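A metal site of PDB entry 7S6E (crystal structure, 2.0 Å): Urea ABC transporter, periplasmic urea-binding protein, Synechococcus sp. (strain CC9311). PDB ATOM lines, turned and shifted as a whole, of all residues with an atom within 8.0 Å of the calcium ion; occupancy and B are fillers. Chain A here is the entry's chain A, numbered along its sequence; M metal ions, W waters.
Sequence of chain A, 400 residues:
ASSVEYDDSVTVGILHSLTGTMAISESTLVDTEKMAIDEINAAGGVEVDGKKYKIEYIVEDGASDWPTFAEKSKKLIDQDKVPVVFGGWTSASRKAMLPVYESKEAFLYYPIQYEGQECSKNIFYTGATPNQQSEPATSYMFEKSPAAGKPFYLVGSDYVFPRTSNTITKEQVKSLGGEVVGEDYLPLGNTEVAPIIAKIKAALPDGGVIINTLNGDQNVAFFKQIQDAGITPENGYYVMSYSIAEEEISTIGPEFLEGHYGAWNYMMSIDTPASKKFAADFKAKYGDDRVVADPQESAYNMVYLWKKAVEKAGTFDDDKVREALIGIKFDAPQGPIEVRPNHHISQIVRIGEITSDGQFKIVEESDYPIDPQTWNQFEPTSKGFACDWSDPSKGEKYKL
The side-chain carboxylate of Asp 318 lies within salt-bridge range of the guanidinium group of Arg 322 (2.8 Å).
The guanidinium group (NH2) of Arg 322 lies close to the side-chain carboxylate (OD1) of Asp 319, at 3.5 Å.
OE2 of Glu 105 lies within hydrogen-bond range of ND2 of Asn 122, at 3.1 Å.
The side-chain carboxylate (OD1) of Asp 317 lies within hydrogen-bond range of the backbone NH (N) of Asp 319, 3.1 Å away.
The side-chain carboxylate (OE2) of Glu 105 lies within salt-bridge range of the guanidinium group (NH2) of Arg 322.
Along chain A the residues within 4 Å of the calcium ion span positions 105 to 319.
The nearest printed residue that does not touch the calcium ion is Arg 322 (4.3 Å).
The calcium ion is bound by the side-chain carboxylate of Asp 318, the backbone carbonyl oxygen of Glu 105, water W1 and the side-chain carboxylate of Asp 319.
The calcium ion has four donor atoms within binding distance.
Slightly farther from the calcium ion lies OD2 of Asp 318 (3.0 Å).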
ATOM      1  N   ILE A  77      16.242 -21.665  -8.848  1.00  0.00           N
ATOM      2  CA  ILE A  77      14.990 -22.269  -8.317  1.00  0.00           C
ATOM      3  C   ILE A  77      13.854 -22.107  -9.342  1.00  0.00           C
ATOM      4  O   ILE A  77      13.317 -23.127  -9.782  1.00  0.00           O
ATOM      5  CB  ILE A  77      14.582 -21.708  -6.953  1.00  0.00           C
ATOM      6  CG1 ILE A  77      15.665 -21.962  -5.885  1.00  0.00           C
ATOM      7  CG2 ILE A  77      13.217 -22.272  -6.558  1.00  0.00           C
ATOM      8  CD1 ILE A  77      15.620 -21.007  -4.712  1.00  0.00           C
ATOM      9  N   VAL A  82      15.889 -26.403 -10.483  1.00  0.00           N
ATOM     10  CA  VAL A  82      16.813 -27.455  -9.982  1.00  0.00           C
ATOM     11  C   VAL A  82      16.187 -28.034  -8.718  1.00  0.00           C
ATOM     12  O   VAL A  82      15.552 -27.331  -7.947  1.00  0.00           O
ATOM     13  CB  VAL A  82      18.245 -26.895  -9.785  1.00  0.00           C
ATOM     14  CG1 VAL A  82      18.779 -26.356 -11.098  1.00  0.00           C
ATOM     15  CG2 VAL A  82      18.312 -25.839  -8.687  1.00  0.00           C
ATOM     16  N   PRO A  83      16.359 -29.341  -8.425  1.00  0.00           N
ATOM     17  CA  PRO A  83      15.895 -29.864  -7.133  1.00  0.00           C
ATOM     18  C   PRO A  83      16.805 -29.519  -5.930  1.00  0.00           C
ATOM     19  O   PRO A  83      16.410 -29.785  -4.777  1.00  0.00           O
ATOM     20  CB  PRO A  83      15.895 -31.372  -7.369  1.00  0.00           C
ATOM     21  CG  PRO A  83      16.957 -31.583  -8.421  1.00  0.00           C
ATOM     22  CD  PRO A  83      16.966 -30.350  -9.289  1.00  0.00           C
ATOM     23  N   TYR A 101      15.523 -19.523  -0.321  1.00  0.00           N
ATOM     24  CA  TYR A 101      15.329 -20.992  -0.244  1.00  0.00           C
ATOM     25  C   TYR A 101      14.173 -21.281   0.737  1.00  0.00           C
ATOM     26  O   TYR A 101      13.440 -22.274   0.486  1.00  0.00           O
ATOM     27  CB  TYR A 101      16.635 -21.709   0.118  1.00  0.00           C
ATOM     28  CG  TYR A 101      17.657 -21.694  -0.977  1.00  0.00           C
ATOM     29  CD1 TYR A 101      17.678 -22.676  -1.952  1.00  0.00           C
ATOM     30  CD2 TYR A 101      18.565 -20.652  -1.084  1.00  0.00           C
ATOM     31  CE1 TYR A 101      18.581 -22.630  -3.012  1.00  0.00           C
ATOM     32  CE2 TYR A 101      19.489 -20.591  -2.121  1.00  0.00           C
ATOM     33  CZ  TYR A 101      19.501 -21.601  -3.072  1.00  0.00           C
ATOM     34  OH  TYR A 101      20.400 -21.525  -4.078  1.00  0.00           O
ATOM     35  N   LYS A 104      10.665 -19.913  -0.988  1.00  0.00           N
ATOM     36  CA  LYS A 104      10.314 -20.727  -2.169  1.00  0.00           C
ATOM     37  C   LYS A 104      10.319 -22.207  -1.796  1.00  0.00           C
ATOM     38  O   LYS A 104      10.128 -23.019  -2.714  1.00  0.00           O
ATOM     39  CB  LYS A 104      11.315 -20.512  -3.298  1.00  0.00           C
ATOM     40  CG  LYS A 104      11.298 -19.083  -3.816  1.00  0.00           C
ATOM     41  CD  LYS A 104      12.202 -18.848  -4.932  1.00  0.00           C
ATOM     42  CE  LYS A 104      12.223 -17.384  -5.335  1.00  0.00           C
ATOM     43  NZ  LYS A 104      10.933 -17.026  -5.973  1.00  0.00           N
ATOM     44  N   GLU A 105      10.527 -22.509  -0.508  1.00  0.00           N
ATOM     45  CA  GLU A 105      10.577 -23.910   0.031  1.00  0.00           C
ATOM     46  C   GLU A 105      11.411 -24.775  -0.925  1.00  0.00           C
ATOM     47  O   GLU A 105      10.886 -25.829  -1.413  1.00  0.00           O
ATOM     48  CB  GLU A 105       9.177 -24.522   0.200  1.00  0.00           C
ATOM     49  CG  GLU A 105       9.180 -25.751   1.131  1.00  0.00           C
ATOM     50  CD  GLU A 105       9.516 -25.462   2.607  1.00  0.00           C
ATOM     51  OE1 GLU A 105       9.167 -24.357   3.105  1.00  0.00           O
ATOM     52  OE2 GLU A 105      10.099 -26.345   3.261  1.00  0.00           O
ATOM     53  N   ALA A 106      12.636 -24.316  -1.193  1.00  0.00           N
ATOM     54  CA  ALA A 106      13.640 -25.043  -2.018  1.00  0.00           C
ATOM     55  C   ALA A 106      14.755 -25.573  -1.098  1.00  0.00           C
ATOM     56  O   ALA A 106      14.456 -25.837   0.137  1.00  0.00           O
ATOM     57  CB  ALA A 106      14.132 -24.138  -3.127  1.00  0.00           C
ATOM     58  N   PHE A 107      15.945 -25.850  -1.658  1.00  0.00           N
ATOM     59  CA  PHE A 107      16.996 -26.627  -0.938  1.00  0.00           C
ATOM     60  C   PHE A 107      18.399 -26.137  -1.338  1.00  0.00           C
ATOM     61  O   PHE A 107      18.833 -26.373  -2.476  1.00  0.00           O
ATOM     62  CB  PHE A 107      16.738 -28.117  -1.196  1.00  0.00           C
ATOM     63  CG  PHE A 107      17.722 -29.119  -0.652  1.00  0.00           C
ATOM     64  CD1 PHE A 107      18.678 -28.742   0.273  1.00  0.00           C
ATOM     65  CD2 PHE A 107      17.723 -30.437  -1.113  1.00  0.00           C
ATOM     66  CE1 PHE A 107      19.600 -29.656   0.733  1.00  0.00           C
ATOM     67  CE2 PHE A 107      18.611 -31.366  -0.621  1.00  0.00           C
ATOM     68  CZ  PHE A 107      19.575 -30.962   0.280  1.00  0.00           C
ATOM     69  N   ASN A 122      15.397 -25.423   5.093  1.00  0.00           N
ATOM     70  CA  ASN A 122      15.664 -25.467   3.632  1.00  0.00           C
ATOM     71  C   ASN A 122      17.181 -25.495   3.343  1.00  0.00           C
ATOM     72  O   ASN A 122      17.554 -25.351   2.165  1.00  0.00           O
ATOM     73  CB  ASN A 122      14.969 -24.288   2.965  1.00  0.00           C
ATOM     74  CG  ASN A 122      13.471 -24.374   3.179  1.00  0.00           C
ATOM     75  OD1 ASN A 122      12.936 -23.783   4.132  1.00  0.00           O
ATOM     76  ND2 ASN A 122      12.831 -25.177   2.354  1.00  0.00           N
ATOM     77  N   PHE A 316      13.354 -36.902  -6.626  1.00  0.00           N
ATOM     78  CA  PHE A 316      14.168 -35.666  -6.599  1.00  0.00           C
ATOM     79  C   PHE A 316      13.438 -34.562  -5.845  1.00  0.00           C
ATOM     80  O   PHE A 316      14.085 -33.569  -5.518  1.00  0.00           O
ATOM     81  CB  PHE A 316      14.484 -35.194  -8.027  1.00  0.00           C
ATOM     82  CG  PHE A 316      15.321 -36.167  -8.802  1.00  0.00           C
ATOM     83  CD1 PHE A 316      16.640 -36.389  -8.456  1.00  0.00           C
ATOM     84  CD2 PHE A 316      14.796 -36.885  -9.872  1.00  0.00           C
ATOM     85  CE1 PHE A 316      17.430 -37.270  -9.179  1.00  0.00           C
ATOM     86  CE2 PHE A 316      15.590 -37.778 -10.574  1.00  0.00           C
ATOM     87  CZ  PHE A 316      16.905 -37.959 -10.241  1.00  0.00           C
ATOM     88  N   ASP A 317      12.152 -34.721  -5.560  1.00  0.00           N
ATOM     89  CA  ASP A 317      11.329 -33.717  -4.833  1.00  0.00           C
ATOM     90  C   ASP A 317      12.080 -33.246  -3.568  1.00  0.00           C
ATOM     91  O   ASP A 317      12.273 -34.078  -2.654  1.00  0.00           O
ATOM     92  CB  ASP A 317       9.960 -34.298  -4.467  1.00  0.00           C
ATOM     93  CG  ASP A 317       9.040 -33.351  -3.720  1.00  0.00           C
ATOM     94  OD1 ASP A 317       9.455 -32.221  -3.434  1.00  0.00           O
ATOM     95  OD2 ASP A 317       7.910 -33.760  -3.456  1.00  0.00           O
ATOM     96  N   ASP A 318      12.470 -31.972  -3.514  1.00  0.00           N
ATOM     97  CA  ASP A 318      13.329 -31.478  -2.389  1.00  0.00           C
ATOM     98  C   ASP A 318      12.599 -31.653  -1.051  1.00  0.00           C
ATOM     99  O   ASP A 318      13.286 -31.869  -0.090  1.00  0.00           O
ATOM    100  CB  ASP A 318      13.790 -30.052  -2.633  1.00  0.00           C
ATOM    101  CG  ASP A 318      12.685 -29.039  -2.472  1.00  0.00           C
ATOM    102  OD1 ASP A 318      11.855 -28.957  -3.387  1.00  0.00           O
ATOM    103  OD2 ASP A 318      12.663 -28.372  -1.408  1.00  0.00           O
ATOM    104  N   ASP A 319      11.258 -31.550  -1.002  1.00  0.00           N
ATOM    105  CA  ASP A 319      10.442 -31.752   0.236  1.00  0.00           C
ATOM    106  C   ASP A 319      10.763 -33.139   0.807  1.00  0.00           C
ATOM    107  O   ASP A 319      11.159 -33.203   1.973  1.00  0.00           O
ATOM    108  CB  ASP A 319       8.953 -31.476   0.014  1.00  0.00           C
ATOM    109  CG  ASP A 319       8.585 -30.000  -0.167  1.00  0.00           C
ATOM    110  OD1 ASP A 319       9.271 -29.270  -0.953  1.00  0.00           O
ATOM    111  OD2 ASP A 319       7.642 -29.557   0.524  1.00  0.00           O
ATOM    112  N   LYS A 320      10.729 -34.195   0.009  1.00  0.00           N
ATOM    113  CA  LYS A 320      10.966 -35.590   0.457  1.00  0.00           C
ATOM    114  C   LYS A 320      12.460 -35.868   0.634  1.00  0.00           C
ATOM    115  O   LYS A 320      12.882 -36.641   1.564  1.00  0.00           O
ATOM    116  CB  LYS A 320      10.319 -36.571  -0.525  1.00  0.00           C
ATOM    117  CG  LYS A 320       8.821 -36.367  -0.687  1.00  0.00           C
ATOM    118  CD  LYS A 320       8.046 -36.569   0.591  1.00  0.00           C
ATOM    119  CE  LYS A 320       6.536 -36.611   0.369  1.00  0.00           C
ATOM    120  NZ  LYS A 320       5.803 -35.806   1.383  1.00  0.00           N
ATOM    121  N   ARG A 322      14.749 -33.701   1.580  1.00  0.00           N
ATOM    122  CA  ARG A 322      15.175 -33.019   2.826  1.00  0.00           C
ATOM    123  C   ARG A 322      14.702 -33.850   4.034  1.00  0.00           C
ATOM    124  O   ARG A 322      15.461 -33.985   4.976  1.00  0.00           O
ATOM    125  CB  ARG A 322      14.708 -31.565   2.812  1.00  0.00           C
ATOM    126  CG  ARG A 322      15.602 -30.635   1.993  1.00  0.00           C
ATOM    127  CD  ARG A 322      15.270 -29.145   2.177  1.00  0.00           C
ATOM    128  NE  ARG A 322      14.040 -28.770   1.493  1.00  0.00           N
ATOM    129  CZ  ARG A 322      12.823 -28.659   2.050  1.00  0.00           C
ATOM    130  NH1 ARG A 322      12.646 -28.796   3.357  1.00  0.00           N
ATOM    131  NH2 ARG A 322      11.795 -28.358   1.277  1.00  0.00           N
HETATM  132 CA    CA M   1      10.077 -27.654  -2.638  1.00  0.00          CA
HETATM  133  O   HOH W   1       8.435 -25.921  -3.191  1.00  0.00           O
